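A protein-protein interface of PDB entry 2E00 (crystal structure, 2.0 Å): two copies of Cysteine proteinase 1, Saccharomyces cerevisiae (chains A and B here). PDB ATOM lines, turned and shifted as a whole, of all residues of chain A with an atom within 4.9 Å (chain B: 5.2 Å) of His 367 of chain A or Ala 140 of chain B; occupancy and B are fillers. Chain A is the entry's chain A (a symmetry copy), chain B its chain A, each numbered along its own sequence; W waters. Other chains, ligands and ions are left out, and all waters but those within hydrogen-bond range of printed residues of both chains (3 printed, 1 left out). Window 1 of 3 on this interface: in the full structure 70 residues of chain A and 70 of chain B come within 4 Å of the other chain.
Among the printed residues, merely in contact across the chains: Tyr 366 of chain A with Arg 189 of chain B (3.3 Å), His 367 of chain A with Gln 136 of chain B (3.5 Å), His 367 of chain A with Ala 140 of chain B (3.6 Å), His 367 of chain A with Leu 139 of chain B (3.7 Å) and Tyr 366 of chain A with Leu 139 of chain B (3.97 Å).
NE of Arg 189 of chain B is in hydrogen-bond range of O of Leu 139 of chain B.
The backbone carbonyl oxygen (O) of Ala 140 of chain B is in hydrogen-bond range of the guanidinium group (NH2) of Arg 189 of chain B (3.0 Å).
The backbone NH (N) of Glu 368 of chain A lies within hydrogen-bond range of the backbone carbonyl oxygen (O) of Arg 363 of chain A (2.9 Å).
His 367 of chain A touches four residues of chain B.
Of chain A, only His 367 (3.6 Å) comes within 4 Å of Ala 140 of chain B.
Printed residues of chain B within 4 Å of Glu 368 of chain A: Arg 189 (2.8 Å).
Printed residues of chain A within 4 Å of Gln 136 of chain B: Arg 365 (3.0 Å) and His 367 (3.5 Å).
Thr 185 of chain B touches none of the printed residues of chain A.
Ile 364 of chain A touches none of the printed residues of chain B.
The nearest printed residue of chain B that does not touch His 367 of chain A is Tyr 137 of chain B (5.6 Å).
The nearest printed residue of chain A that does not touch Ala 140 of chain B is Tyr 366 of chain A (6.3 Å).
O of His 367 of chain A sits close to NH1 of Arg 189 of chain B (3.2 Å).
The guanidinium group (NH1) of Arg 189 of chain B lies within salt-bridge range of the side-chain carboxylate (OE1) of Glu 368 of chain A, 2.8 Å away.
The side-chain amide nitrogen (NE2) of Gln 136 of chain B is in hydrogen-bond range of the backbone carbonyl oxygen (O) of Arg 365 of chain A, at 3.0 Å.
Of the 7 printed residues of chain A, 4 touch a printed residue of chain B.
Printed residues of chain A that touch a printed residue of chain B: Arg 365, Tyr 366, His 367 and Glu 368.
Hydrophobic or aromatic side chains of chain A that line the printed part of chain B: Tyr 366 and His 367.
Along chain A the printed residues that touch a printed residue of chain B span positions 365 to 368.
Of the 9 printed residues of chain B, 4 touch a printed residue of chain A.
Along chain B the printed residues that touch a printed residue of chain A span positions 136 to 189.
Among the printed residues, 8 pairs touch across the chains.
Among the printed residues, Asp or Glu carboxylates within 4 Å of a Lys or Arg side-chain nitrogen of the other chain: Glu 368 of chain A with Arg 189 of chain B (2.8 Å).
No position is printed for both chains.
Water W3 bridges the backbone carbonyl oxygen of Glu 368 of chain A (2.9 Å) and the guanidinium group of Arg 189 of chain B (3.2 Å).
Water W2 lies within hydrogen-bond range of the backbone carbonyl oxygen (O) of Arg 365 of chain A and the side-chain amide nitrogen (NE2) of Gln 136 of chain B.
Water W1 bridges NH1 of Arg 189 of chain B (3.3 Å) and OE1 of Glu 368 of chain A (3.4 Å).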
ATOM      1  N   ARG A 363      14.852  10.196  12.947  1.00  0.00           N
ATOM      2  CA  ARG A 363      14.526   9.232  13.994  1.00  0.00           C
ATOM      3  C   ARG A 363      13.449   8.281  13.460  1.00  0.00           C
ATOM      4  O   ARG A 363      13.481   7.075  13.719  1.00  0.00           O
ATOM      5  CB  ARG A 363      14.013   9.949  15.251  1.00  0.00           C
ATOM      6  CG  ARG A 363      15.102  10.419  16.215  1.00  0.00           C
ATOM      7  CD  ARG A 363      14.499  11.067  17.460  1.00  0.00           C
ATOM      8  NE  ARG A 363      14.066  12.440  17.208  1.00  0.00           N
ATOM      9  CZ  ARG A 363      12.983  12.996  17.735  1.00  0.00           C
ATOM     10  NH1 ARG A 363      12.210  12.307  18.547  1.00  0.00           N
ATOM     11  NH2 ARG A 363      12.656  14.234  17.439  1.00  0.00           N
ATOM     12  N   ILE A 364      12.530   8.829  12.667  1.00  0.00           N
ATOM     13  CA  ILE A 364      11.458   8.032  12.099  1.00  0.00           C
ATOM     14  C   ILE A 364      11.993   7.079  11.033  1.00  0.00           C
ATOM     15  O   ILE A 364      11.722   5.881  11.083  1.00  0.00           O
ATOM     16  CB  ILE A 364      10.353   8.919  11.503  1.00  0.00           C
ATOM     17  CG1 ILE A 364       9.725   9.781  12.603  1.00  0.00           C
ATOM     18  CG2 ILE A 364       9.287   8.053  10.847  1.00  0.00           C
ATOM     19  CD1 ILE A 364       8.708  10.789  12.097  1.00  0.00           C
ATOM     20  N   ARG A 365      12.786   7.607  10.101  1.00  0.00           N
ATOM     21  CA  ARG A 365      13.358   6.797   9.024  1.00  0.00           C
ATOM     22  C   ARG A 365      14.296   5.716   9.540  1.00  0.00           C
ATOM     23  O   ARG A 365      14.310   4.605   9.016  1.00  0.00           O
ATOM     24  CB  ARG A 365      14.151   7.662   8.031  1.00  0.00           C
ATOM     25  CG  ARG A 365      13.367   8.729   7.290  1.00  0.00           C
ATOM     26  CD  ARG A 365      14.272   9.408   6.261  1.00  0.00           C
ATOM     27  NE  ARG A 365      13.766  10.701   5.798  1.00  0.00           N
ATOM     28  CZ  ARG A 365      12.854  10.858   4.842  1.00  0.00           C
ATOM     29  NH1 ARG A 365      12.326   9.801   4.234  1.00  0.00           N
ATOM     30  NH2 ARG A 365      12.483  12.080   4.481  1.00  0.00           N
ATOM     31  N   TYR A 366      15.074   6.045  10.572  1.00  0.00           N
ATOM     32  CA  TYR A 366      16.044   5.100  11.121  1.00  0.00           C
ATOM     33  C   TYR A 366      15.589   4.119  12.191  1.00  0.00           C
ATOM     34  O   TYR A 366      16.407   3.600  12.957  1.00  0.00           O
ATOM     35  CB  TYR A 366      17.342   5.816  11.515  1.00  0.00           C
ATOM     36  CG  TYR A 366      18.186   6.141  10.302  1.00  0.00           C
ATOM     37  CD1 TYR A 366      17.854   7.208   9.466  1.00  0.00           C
ATOM     38  CD2 TYR A 366      19.271   5.338   9.947  1.00  0.00           C
ATOM     39  CE1 TYR A 366      18.574   7.462   8.301  1.00  0.00           C
ATOM     40  CE2 TYR A 366      19.999   5.581   8.784  1.00  0.00           C
ATOM     41  CZ  TYR A 366      19.641   6.642   7.966  1.00  0.00           C
ATOM     42  OH  TYR A 366      20.329   6.869   6.800  1.00  0.00           O
ATOM     43  N   HIS A 367      14.286   3.834  12.211  1.00  0.00           N
ATOM     44  CA  HIS A 367      13.725   2.849  13.140  1.00  0.00           C
ATOM     45  C   HIS A 367      13.817   3.224  14.620  1.00  0.00           C
ATOM     46  O   HIS A 367      13.645   2.367  15.487  1.00  0.00           O
ATOM     47  CB  HIS A 367      14.431   1.508  12.904  1.00  0.00           C
ATOM     48  CG  HIS A 367      13.574   0.307  13.149  1.00  0.00           C
ATOM     49  ND1 HIS A 367      13.000   0.032  14.371  1.00  0.00           N
ATOM     50  CD2 HIS A 367      13.213  -0.708  12.325  1.00  0.00           C
ATOM     51  CE1 HIS A 367      12.323  -1.098  14.291  1.00  0.00           C
ATOM     52  NE2 HIS A 367      12.437  -1.567  13.061  1.00  0.00           N
ATOM     53  N   GLU A 368      14.055   4.498  14.916  1.00  0.00           N
ATOM     54  CA  GLU A 368      14.178   4.932  16.303  1.00  0.00           C
ATOM     55  C   GLU A 368      12.896   5.418  16.971  1.00  0.00           C
ATOM     56  O   GLU A 368      12.710   5.208  18.170  1.00  0.00           O
ATOM     57  CB  GLU A 368      15.267   6.000  16.440  1.00  0.00           C
ATOM     58  CG  GLU A 368      15.416   6.592  17.851  1.00  0.00           C
ATOM     59  CD  GLU A 368      15.690   5.548  18.933  1.00  0.00           C
ATOM     60  OE1 GLU A 368      16.249   4.480  18.628  1.00  0.00           O
ATOM     61  OE2 GLU A 368      15.358   5.808  20.105  1.00  0.00           O
ATOM     62  N   SER A 369      12.023   6.076  16.214  1.00  0.00           N
ATOM     63  CA  SER A 369      10.791   6.589  16.797  1.00  0.00           C
ATOM     64  C   SER A 369       9.572   6.319  15.924  1.00  0.00           C
ATOM     65  O   SER A 369       9.656   6.319  14.695  1.00  0.00           O
ATOM     66  CB  SER A 369      10.927   8.082  17.096  1.00  0.00           C
ATOM     67  OG  SER A 369       9.922   8.517  17.994  1.00  0.00           O
ATOM     68  N   GLN B 136      16.267  -1.791   7.053  1.00  0.00           N
ATOM     69  CA  GLN B 136      15.304  -1.689   8.141  1.00  0.00           C
ATOM     70  C   GLN B 136      15.479  -2.847   9.123  1.00  0.00           C
ATOM     71  O   GLN B 136      15.389  -2.654  10.339  1.00  0.00           O
ATOM     72  CB  GLN B 136      13.870  -1.633   7.595  1.00  0.00           C
ATOM     73  CG  GLN B 136      13.494  -0.248   7.062  1.00  0.00           C
ATOM     74  CD  GLN B 136      13.628   0.839   8.118  1.00  0.00           C
ATOM     75  OE1 GLN B 136      13.046   0.742   9.197  1.00  0.00           O
ATOM     76  NE2 GLN B 136      14.393   1.884   7.810  1.00  0.00           N
ATOM     77  N   TYR B 137      15.775  -4.037   8.601  1.00  0.00           N
ATOM     78  CA  TYR B 137      15.984  -5.195   9.460  1.00  0.00           C
ATOM     79  C   TYR B 137      17.239  -5.008  10.315  1.00  0.00           C
ATOM     80  O   TYR B 137      17.265  -5.399  11.480  1.00  0.00           O
ATOM     81  CB  TYR B 137      16.101  -6.492   8.654  1.00  0.00           C
ATOM     82  CG  TYR B 137      16.237  -7.707   9.548  1.00  0.00           C
ATOM     83  CD1 TYR B 137      15.110  -8.334  10.081  1.00  0.00           C
ATOM     84  CD2 TYR B 137      17.492  -8.181   9.924  1.00  0.00           C
ATOM     85  CE1 TYR B 137      15.234  -9.401  10.973  1.00  0.00           C
ATOM     86  CE2 TYR B 137      17.626  -9.240  10.816  1.00  0.00           C
ATOM     87  CZ  TYR B 137      16.496  -9.844  11.338  1.00  0.00           C
ATOM     88  OH  TYR B 137      16.631 -10.878  12.236  1.00  0.00           O
ATOM     89  N   LEU B 138      18.283  -4.428   9.726  1.00  0.00           N
ATOM     90  CA  LEU B 138      19.532  -4.188  10.455  1.00  0.00           C
ATOM     91  C   LEU B 138      19.324  -3.198  11.601  1.00  0.00           C
ATOM     92  O   LEU B 138      19.893  -3.353  12.682  1.00  0.00           O
ATOM     93  CB  LEU B 138      20.615  -3.656   9.507  1.00  0.00           C
ATOM     94  CG  LEU B 138      21.175  -4.674   8.509  1.00  0.00           C
ATOM     95  CD1 LEU B 138      22.057  -3.974   7.480  1.00  0.00           C
ATOM     96  CD2 LEU B 138      21.949  -5.773   9.260  1.00  0.00           C
ATOM     97  N   LEU B 139      18.465  -2.212  11.367  1.00  0.00           N
ATOM     98  CA  LEU B 139      18.167  -1.174  12.352  1.00  0.00           C
ATOM     99  C   LEU B 139      17.195  -1.590  13.459  1.00  0.00           C
ATOM    100  O   LEU B 139      17.080  -0.906  14.475  1.00  0.00           O
ATOM    101  CB  LEU B 139      17.597   0.054  11.634  1.00  0.00           C
ATOM    102  CG  LEU B 139      18.512   0.777  10.643  1.00  0.00           C
ATOM    103  CD1 LEU B 139      17.689   1.676   9.730  1.00  0.00           C
ATOM    104  CD2 LEU B 139      19.562   1.580  11.395  1.00  0.00           C
ATOM    105  N   ALA B 140      16.498  -2.702  13.255  1.00  0.00           N
ATOM    106  CA  ALA B 140      15.503  -3.193  14.207  1.00  0.00           C
ATOM    107  C   ALA B 140      16.024  -3.583  15.592  1.00  0.00           C
ATOM    108  O   ALA B 140      15.468  -3.147  16.599  1.00  0.00           O
ATOM    109  CB  ALA B 140      14.716  -4.348  13.593  1.00  0.00           C
ATOM    110  N   ALA B 141      17.076  -4.397  15.645  1.00  0.00           N
ATOM    111  CA  ALA B 141      17.636  -4.842  16.925  1.00  0.00           C
ATOM    112  C   ALA B 141      19.105  -5.255  16.800  1.00  0.00           C
ATOM    113  O   ALA B 141      19.453  -6.426  16.973  1.00  0.00           O
ATOM    114  CB  ALA B 141      16.805  -6.008  17.481  1.00  0.00           C
ATOM    115  N   PRO B 142      19.993  -4.281  16.553  1.00  0.00           N
ATOM    116  CA  PRO B 142      21.432  -4.524  16.400  1.00  0.00           C
ATOM    117  C   PRO B 142      22.191  -5.075  17.607  1.00  0.00           C
ATOM    118  O   PRO B 142      23.210  -5.745  17.432  1.00  0.00           O
ATOM    119  CB  PRO B 142      21.964  -3.152  15.981  1.00  0.00           C
ATOM    120  CG  PRO B 142      21.021  -2.205  16.667  1.00  0.00           C
ATOM    121  CD  PRO B 142      19.687  -2.850  16.383  1.00  0.00           C
ATOM    122  N   THR B 185      21.400   0.998  21.108  1.00  0.00           N
ATOM    123  CA  THR B 185      20.713   0.947  19.830  1.00  0.00           C
ATOM    124  C   THR B 185      20.325   2.327  19.307  1.00  0.00           C
ATOM    125  O   THR B 185      20.429   2.591  18.106  1.00  0.00           O
ATOM    126  CB  THR B 185      19.497   0.016  19.923  1.00  0.00           C
ATOM    127  OG1 THR B 185      19.962  -1.304  20.226  1.00  0.00           O
ATOM    128  CG2 THR B 185      18.723  -0.010  18.611  1.00  0.00           C
ATOM    129  N   ARG B 189      21.621   3.789  15.772  1.00  0.00           N
ATOM    130  CA  ARG B 189      20.718   4.289  14.730  1.00  0.00           C
ATOM    131  C   ARG B 189      21.172   5.683  14.291  1.00  0.00           C
ATOM    132  O   ARG B 189      21.060   6.042  13.118  1.00  0.00           O
ATOM    133  CB  ARG B 189      19.264   4.294  15.222  1.00  0.00           C
ATOM    134  CG  ARG B 189      18.678   2.873  15.328  1.00  0.00           C
ATOM    135  CD  ARG B 189      17.325   2.844  16.033  1.00  0.00           C
ATOM    136  NE  ARG B 189      16.753   1.494  16.089  1.00  0.00           N
ATOM    137  CZ  ARG B 189      15.926   1.066  17.045  1.00  0.00           C
ATOM    138  NH1 ARG B 189      15.565   1.871  18.038  1.00  0.00           N
ATOM    139  NH2 ARG B 189      15.454  -0.170  17.010  1.00  0.00           N
HETATM  140  O   HOH W   1      16.515   2.293  21.172  1.00  0.00           O
HETATM  141  O   HOH W   2      12.057   3.795   7.150  1.00  0.00           O
HETATM  142  O   HOH W   3      13.257   3.005  19.949  1.00  0.00           O
